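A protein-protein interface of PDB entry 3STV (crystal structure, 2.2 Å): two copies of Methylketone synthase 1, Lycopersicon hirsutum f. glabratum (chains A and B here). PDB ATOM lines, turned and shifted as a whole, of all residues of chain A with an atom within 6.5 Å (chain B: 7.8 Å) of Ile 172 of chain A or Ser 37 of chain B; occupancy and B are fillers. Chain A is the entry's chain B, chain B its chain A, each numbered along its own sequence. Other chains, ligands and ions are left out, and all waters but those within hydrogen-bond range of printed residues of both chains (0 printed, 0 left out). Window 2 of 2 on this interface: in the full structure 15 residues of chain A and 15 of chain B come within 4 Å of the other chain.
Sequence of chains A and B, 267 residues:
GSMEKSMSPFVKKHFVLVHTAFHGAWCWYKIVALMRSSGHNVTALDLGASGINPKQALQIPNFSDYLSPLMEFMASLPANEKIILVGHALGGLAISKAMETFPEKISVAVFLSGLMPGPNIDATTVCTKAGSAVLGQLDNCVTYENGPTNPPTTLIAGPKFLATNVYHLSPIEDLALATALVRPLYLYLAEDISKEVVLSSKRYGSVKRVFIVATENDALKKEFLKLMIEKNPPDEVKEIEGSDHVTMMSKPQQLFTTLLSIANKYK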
ATOM      1  N   SER A 170      -6.547  -5.759 -23.614  1.00  0.00           N
ATOM      2  CA  SER A 170      -6.414  -4.541 -22.826  1.00  0.00           C
ATOM      3  C   SER A 170      -7.465  -4.486 -21.734  1.00  0.00           C
ATOM      4  O   SER A 170      -8.472  -5.186 -21.804  1.00  0.00           O
ATOM      5  CB  SER A 170      -6.569  -3.310 -23.726  1.00  0.00           C
ATOM      6  OG  SER A 170      -5.669  -3.355 -24.818  1.00  0.00           O
ATOM      7  N   PRO A 171      -7.231  -3.658 -20.701  1.00  0.00           N
ATOM      8  CA  PRO A 171      -8.158  -3.485 -19.574  1.00  0.00           C
ATOM      9  C   PRO A 171      -9.527  -3.082 -20.128  1.00  0.00           C
ATOM     10  O   PRO A 171      -9.605  -2.297 -21.074  1.00  0.00           O
ATOM     11  CB  PRO A 171      -7.518  -2.354 -18.781  1.00  0.00           C
ATOM     12  CG  PRO A 171      -6.064  -2.573 -19.010  1.00  0.00           C
ATOM     13  CD  PRO A 171      -5.988  -2.896 -20.482  1.00  0.00           C
ATOM     14  N   ILE A 172     -10.602  -3.600 -19.550  1.00  0.00           N
ATOM     15  CA  ILE A 172     -11.929  -3.261 -20.054  1.00  0.00           C
ATOM     16  C   ILE A 172     -12.191  -1.763 -20.091  1.00  0.00           C
ATOM     17  O   ILE A 172     -12.879  -1.286 -20.991  1.00  0.00           O
ATOM     18  CB  ILE A 172     -13.052  -3.954 -19.248  1.00  0.00           C
ATOM     19  CG1 ILE A 172     -12.826  -3.765 -17.751  1.00  0.00           C
ATOM     20  CG2 ILE A 172     -13.097  -5.426 -19.607  1.00  0.00           C
ATOM     21  CD1 ILE A 172     -13.939  -4.330 -16.893  1.00  0.00           C
ATOM     22  N   GLU A 173     -11.635  -1.017 -19.137  1.00  0.00           N
ATOM     23  CA  GLU A 173     -11.849   0.429 -19.116  1.00  0.00           C
ATOM     24  C   GLU A 173     -11.258   1.113 -20.348  1.00  0.00           C
ATOM     25  O   GLU A 173     -11.741   2.161 -20.764  1.00  0.00           O
ATOM     26  CB  GLU A 173     -11.263   1.075 -17.850  1.00  0.00           C
ATOM     27  CG  GLU A 173      -9.759   1.002 -17.747  1.00  0.00           C
ATOM     28  CD  GLU A 173      -9.299  -0.112 -16.832  1.00  0.00           C
ATOM     29  OE1 GLU A 173     -10.038  -1.119 -16.712  1.00  0.00           O
ATOM     30  OE2 GLU A 173      -8.201   0.020 -16.243  1.00  0.00           O
ATOM     31  N   ASP A 174     -10.220   0.522 -20.931  1.00  0.00           N
ATOM     32  CA  ASP A 174      -9.603   1.103 -22.124  1.00  0.00           C
ATOM     33  C   ASP A 174     -10.484   0.931 -23.355  1.00  0.00           C
ATOM     34  O   ASP A 174     -10.475   1.775 -24.248  1.00  0.00           O
ATOM     35  CB  ASP A 174      -8.219   0.503 -22.369  1.00  0.00           C
ATOM     36  CG  ASP A 174      -7.228   0.895 -21.295  1.00  0.00           C
ATOM     37  OD1 ASP A 174      -7.261   2.060 -20.857  1.00  0.00           O
ATOM     38  OD2 ASP A 174      -6.415   0.048 -20.885  1.00  0.00           O
ATOM     39  N   LEU A 175     -11.241  -0.163 -23.400  1.00  0.00           N
ATOM     40  CA  LEU A 175     -12.157  -0.402 -24.508  1.00  0.00           C
ATOM     41  C   LEU A 175     -13.312   0.601 -24.373  1.00  0.00           C
ATOM     42  O   LEU A 175     -13.827   1.121 -25.366  1.00  0.00           O
ATOM     43  CB  LEU A 175     -12.696  -1.835 -24.463  1.00  0.00           C
ATOM     44  CG  LEU A 175     -13.928  -2.117 -25.338  1.00  0.00           C
ATOM     45  CD1 LEU A 175     -13.612  -1.811 -26.803  1.00  0.00           C
ATOM     46  CD2 LEU A 175     -14.364  -3.573 -25.168  1.00  0.00           C
ATOM     47  N   ALA A 176     -13.707   0.876 -23.133  1.00  0.00           N
ATOM     48  CA  ALA A 176     -14.785   1.825 -22.864  1.00  0.00           C
ATOM     49  C   ALA A 176     -14.352   3.232 -23.287  1.00  0.00           C
ATOM     50  O   ALA A 176     -15.131   3.972 -23.890  1.00  0.00           O
ATOM     51  CB  ALA A 176     -15.152   1.803 -21.377  1.00  0.00           C
ATOM     52  N   LEU A 177     -13.108   3.590 -22.974  1.00  0.00           N
ATOM     53  CA  LEU A 177     -12.571   4.899 -23.331  1.00  0.00           C
ATOM     54  C   LEU A 177     -12.580   5.054 -24.857  1.00  0.00           C
ATOM     55  O   LEU A 177     -12.990   6.094 -25.394  1.00  0.00           O
ATOM     56  CB  LEU A 177     -11.137   5.046 -22.792  1.00  0.00           C
ATOM     57  CG  LEU A 177     -10.399   6.354 -23.112  1.00  0.00           C
ATOM     58  CD1 LEU A 177     -11.131   7.512 -22.449  1.00  0.00           C
ATOM     59  CD2 LEU A 177      -8.937   6.298 -22.627  1.00  0.00           C
ATOM     60  N   TYR B  29     -15.029   6.925 -18.414  1.00  0.00           N
ATOM     61  CA  TYR B  29     -14.579   5.612 -18.850  1.00  0.00           C
ATOM     62  C   TYR B  29     -14.425   4.522 -17.792  1.00  0.00           C
ATOM     63  O   TYR B  29     -14.773   3.366 -18.047  1.00  0.00           O
ATOM     64  CB  TYR B  29     -13.304   5.735 -19.703  1.00  0.00           C
ATOM     65  CG  TYR B  29     -11.981   5.823 -18.966  1.00  0.00           C
ATOM     66  CD1 TYR B  29     -11.016   4.824 -19.120  1.00  0.00           C
ATOM     67  CD2 TYR B  29     -11.666   6.926 -18.168  1.00  0.00           C
ATOM     68  CE1 TYR B  29      -9.769   4.920 -18.498  1.00  0.00           C
ATOM     69  CE2 TYR B  29     -10.418   7.035 -17.547  1.00  0.00           C
ATOM     70  CZ  TYR B  29      -9.478   6.028 -17.719  1.00  0.00           C
ATOM     71  OH  TYR B  29      -8.249   6.129 -17.116  1.00  0.00           O
ATOM     72  N   LYS B  30     -13.930   4.860 -16.609  1.00  0.00           N
ATOM     73  CA  LYS B  30     -13.774   3.841 -15.575  1.00  0.00           C
ATOM     74  C   LYS B  30     -15.141   3.397 -15.078  1.00  0.00           C
ATOM     75  O   LYS B  30     -15.366   2.213 -14.820  1.00  0.00           O
ATOM     76  CB  LYS B  30     -12.963   4.379 -14.400  1.00  0.00           C
ATOM     77  CG  LYS B  30     -11.497   4.654 -14.712  1.00  0.00           C
ATOM     78  CD  LYS B  30     -10.829   5.375 -13.549  1.00  0.00           C
ATOM     79  CE  LYS B  30      -9.396   5.789 -13.875  1.00  0.00           C
ATOM     80  NZ  LYS B  30      -8.845   6.664 -12.796  1.00  0.00           N
ATOM     81  N   ILE B  31     -16.055   4.354 -14.956  1.00  0.00           N
ATOM     82  CA  ILE B  31     -17.406   4.081 -14.477  1.00  0.00           C
ATOM     83  C   ILE B  31     -18.168   3.246 -15.493  1.00  0.00           C
ATOM     84  O   ILE B  31     -18.822   2.259 -15.144  1.00  0.00           O
ATOM     85  CB  ILE B  31     -18.175   5.400 -14.212  1.00  0.00           C
ATOM     86  CG1 ILE B  31     -17.379   6.263 -13.221  1.00  0.00           C
ATOM     87  CG2 ILE B  31     -19.590   5.106 -13.684  1.00  0.00           C
ATOM     88  CD1 ILE B  31     -17.003   5.549 -11.922  1.00  0.00           C
ATOM     89  N   VAL B  32     -18.069   3.643 -16.757  1.00  0.00           N
ATOM     90  CA  VAL B  32     -18.744   2.923 -17.825  1.00  0.00           C
ATOM     91  C   VAL B  32     -18.285   1.465 -17.845  1.00  0.00           C
ATOM     92  O   VAL B  32     -19.101   0.561 -17.953  1.00  0.00           O
ATOM     93  CB  VAL B  32     -18.469   3.578 -19.207  1.00  0.00           C
ATOM     94  CG1 VAL B  32     -19.047   2.727 -20.310  1.00  0.00           C
ATOM     95  CG2 VAL B  32     -19.089   4.967 -19.252  1.00  0.00           C
ATOM     96  N   ALA B  33     -16.981   1.233 -17.716  1.00  0.00           N
ATOM     97  CA  ALA B  33     -16.473  -0.134 -17.732  1.00  0.00           C
ATOM     98  C   ALA B  33     -17.048  -0.942 -16.577  1.00  0.00           C
ATOM     99  O   ALA B  33     -17.432  -2.101 -16.752  1.00  0.00           O
ATOM    100  CB  ALA B  33     -14.949  -0.135 -17.666  1.00  0.00           C
ATOM    101  N   LEU B  34     -17.115  -0.323 -15.399  1.00  0.00           N
ATOM    102  CA  LEU B  34     -17.638  -0.995 -14.214  1.00  0.00           C
ATOM    103  C   LEU B  34     -19.115  -1.328 -14.327  1.00  0.00           C
ATOM    104  O   LEU B  34     -19.554  -2.385 -13.883  1.00  0.00           O
ATOM    105  CB  LEU B  34     -17.397  -0.140 -12.970  1.00  0.00           C
ATOM    106  CG  LEU B  34     -15.936  -0.102 -12.517  1.00  0.00           C
ATOM    107  CD1 LEU B  34     -15.748   0.955 -11.450  1.00  0.00           C
ATOM    108  CD2 LEU B  34     -15.529  -1.475 -12.003  1.00  0.00           C
ATOM    109  N   MET B  35     -19.886  -0.426 -14.917  1.00  0.00           N
ATOM    110  CA  MET B  35     -21.305  -0.658 -15.069  1.00  0.00           C
ATOM    111  C   MET B  35     -21.537  -1.774 -16.088  1.00  0.00           C
ATOM    112  O   MET B  35     -22.330  -2.691 -15.846  1.00  0.00           O
ATOM    113  CB  MET B  35     -22.004   0.636 -15.502  1.00  0.00           C
ATOM    114  CG  MET B  35     -21.754   1.796 -14.547  1.00  0.00           C
ATOM    115  SD  MET B  35     -22.674   3.303 -14.907  1.00  0.00           S
ATOM    116  CE  MET B  35     -22.987   3.929 -13.230  1.00  0.00           C
ATOM    117  N   ARG B  36     -20.827  -1.717 -17.212  1.00  0.00           N
ATOM    118  CA  ARG B  36     -20.987  -2.732 -18.249  1.00  0.00           C
ATOM    119  C   ARG B  36     -20.562  -4.125 -17.811  1.00  0.00           C
ATOM    120  O   ARG B  36     -21.223  -5.109 -18.152  1.00  0.00           O
ATOM    121  CB  ARG B  36     -20.236  -2.324 -19.520  1.00  0.00           C
ATOM    122  CG  ARG B  36     -20.952  -1.221 -20.263  1.00  0.00           C
ATOM    123  CD  ARG B  36     -20.228  -0.724 -21.495  1.00  0.00           C
ATOM    124  NE  ARG B  36     -20.940   0.431 -22.031  1.00  0.00           N
ATOM    125  CZ  ARG B  36     -20.449   1.280 -22.929  1.00  0.00           C
ATOM    126  NH1 ARG B  36     -19.224   1.116 -23.418  1.00  0.00           N
ATOM    127  NH2 ARG B  36     -21.188   2.305 -23.330  1.00  0.00           N
ATOM    128  N   SER B  37     -19.474  -4.225 -17.055  1.00  0.00           N
ATOM    129  CA  SER B  37     -19.038  -5.541 -16.606  1.00  0.00           C
ATOM    130  C   SER B  37     -20.005  -6.090 -15.554  1.00  0.00           C
ATOM    131  O   SER B  37     -20.035  -7.292 -15.304  1.00  0.00           O
ATOM    132  CB  SER B  37     -17.602  -5.491 -16.064  1.00  0.00           C
ATOM    133  OG  SER B  37     -17.472  -4.551 -15.017  1.00  0.00           O
ATOM    134  N   SER B  38     -20.799  -5.212 -14.948  1.00  0.00           N
ATOM    135  CA  SER B  38     -21.791  -5.635 -13.958  1.00  0.00           C
ATOM    136  C   SER B  38     -23.122  -5.930 -14.643  1.00  0.00           C
ATOM    137  O   SER B  38     -24.123  -6.197 -13.981  1.00  0.00           O
ATOM    138  CB  SER B  38     -22.007  -4.560 -12.895  1.00  0.00           C
ATOM    139  OG  SER B  38     -20.935  -4.539 -11.972  1.00  0.00           O
ATOM    140  N   GLY B  39     -23.130  -5.855 -15.971  1.00  0.00           N
ATOM    141  CA  GLY B  39     -24.338  -6.148 -16.722  1.00  0.00           C
ATOM    142  C   GLY B  39     -25.364  -5.041 -16.890  1.00  0.00           C
ATOM    143  O   GLY B  39     -26.491  -5.309 -17.314  1.00  0.00           O
ATOM    144  N   HIS B  40     -25.007  -3.802 -16.573  1.00  0.00           N
ATOM    145  CA  HIS B  40     -25.960  -2.710 -16.738  1.00  0.00           C
ATOM    146  C   HIS B  40     -25.755  -1.935 -18.018  1.00  0.00           C
ATOM    147  O   HIS B  40     -24.678  -1.961 -18.605  1.00  0.00           O
ATOM    148  CB  HIS B  40     -25.884  -1.726 -15.574  1.00  0.00           C
ATOM    149  CG  HIS B  40     -26.323  -2.308 -14.275  1.00  0.00           C
ATOM    150  ND1 HIS B  40     -25.454  -2.952 -13.423  1.00  0.00           N
ATOM    151  CD2 HIS B  40     -27.546  -2.389 -13.701  1.00  0.00           C
ATOM    152  CE1 HIS B  40     -26.121  -3.400 -12.375  1.00  0.00           C
ATOM    153  NE2 HIS B  40     -27.392  -3.072 -12.519  1.00  0.00           N
ATOM    154  N   VAL B  42     -25.412   1.594 -19.972  1.00  0.00           N
ATOM    155  CA  VAL B  42     -24.924   2.915 -19.619  1.00  0.00           C
ATOM    156  C   VAL B  42     -24.620   3.756 -20.856  1.00  0.00           C
ATOM    157  O   VAL B  42     -24.049   3.274 -21.839  1.00  0.00           O
ATOM    158  CB  VAL B  42     -23.675   2.807 -18.717  1.00  0.00           C
ATOM    159  CG1 VAL B  42     -22.681   1.831 -19.319  1.00  0.00           C
ATOM    160  CG2 VAL B  42     -23.060   4.169 -18.512  1.00  0.00           C
ATOM    161  N   PHE B 256     -18.942   4.328  -8.321  1.00  0.00           N
ATOM    162  CA  PHE B 256     -19.716   3.268  -8.952  1.00  0.00           C
ATOM    163  C   PHE B 256     -20.605   2.580  -7.913  1.00  0.00           C
ATOM    164  O   PHE B 256     -21.801   2.376  -8.138  1.00  0.00           O
ATOM    165  CB  PHE B 256     -18.772   2.238  -9.595  1.00  0.00           C
ATOM    166  CG  PHE B 256     -19.433   0.925  -9.913  1.00  0.00           C
ATOM    167  CD1 PHE B 256     -20.401   0.839 -10.910  1.00  0.00           C
ATOM    168  CD2 PHE B 256     -19.126  -0.215  -9.176  1.00  0.00           C
ATOM    169  CE1 PHE B 256     -21.059  -0.366 -11.167  1.00  0.00           C
ATOM    170  CE2 PHE B 256     -19.774  -1.422  -9.422  1.00  0.00           C
ATOM    171  CZ  PHE B 256     -20.745  -1.497 -10.420  1.00  0.00           C
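No position is printed for both chains.
Of the 5 pairs that touch across the chains among the printed residues, none has its exchanged pair printed and touching as well.
Of the 8 printed residues of chain A, 4 touch a printed residue of chain B.
Printed residues of chain A that touch a printed residue of chain B: Ile 172, Glu 173, Ala 176 and Leu 177.
Hydrophobic or aromatic side chains of chain A within 4 Å of the printed part of chain B: Ile 172, Ala 176 and Leu 177.
Along chain A the printed residues that touch a printed residue of chain B span positions 172 to 177.
Of the 14 printed residues of chain B, 3 touch a printed residue of chain A.
Among the printed residues, 5 pairs touch across the chains.
Printed residues of chain B within 4 Å of Ile 172 of chain A: Ser 37 (3.9 Å).
Of the printed residues of chain B, Ala 176 of chain A touches Tyr 29 (3.7 Å).
Of the printed residues of chain A, Ala 33 of chain B touches Glu 173.
Ser 37 of chain B touches just one residue of chain A: Ile 172.
The nearest printed residue of chain A that does not touch Ser 37 of chain B is Glu 173 of chain A (8.0 Å).
The nearest printed residue of chain B that does not touch Leu 177 of chain A is Lys 30 of chain B (6.5 Å).
The side-chain hydroxyl (OG) of Ser 37 of chain B is in hydrogen-bond range of the backbone carbonyl oxygen (O) of Ala 33 of chain B.
The backbone carbonyl oxygen (O) of Leu 34 of chain B is in hydrogen-bond range of the side-chain hydroxyl (OG) of Ser 37 of chain B (3.2 Å).
Among the printed residues, merely in contact across the chains: Glu 173 of chain A with Tyr 29 of chain B, Glu 173 of chain A with Ala 33 of chain B, Leu 177 of chain A with Tyr 29 of chain B, Ala 176 of chain A with Tyr 29 of chain B and Ile 172 of chain A with Ser 37 of chain B.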
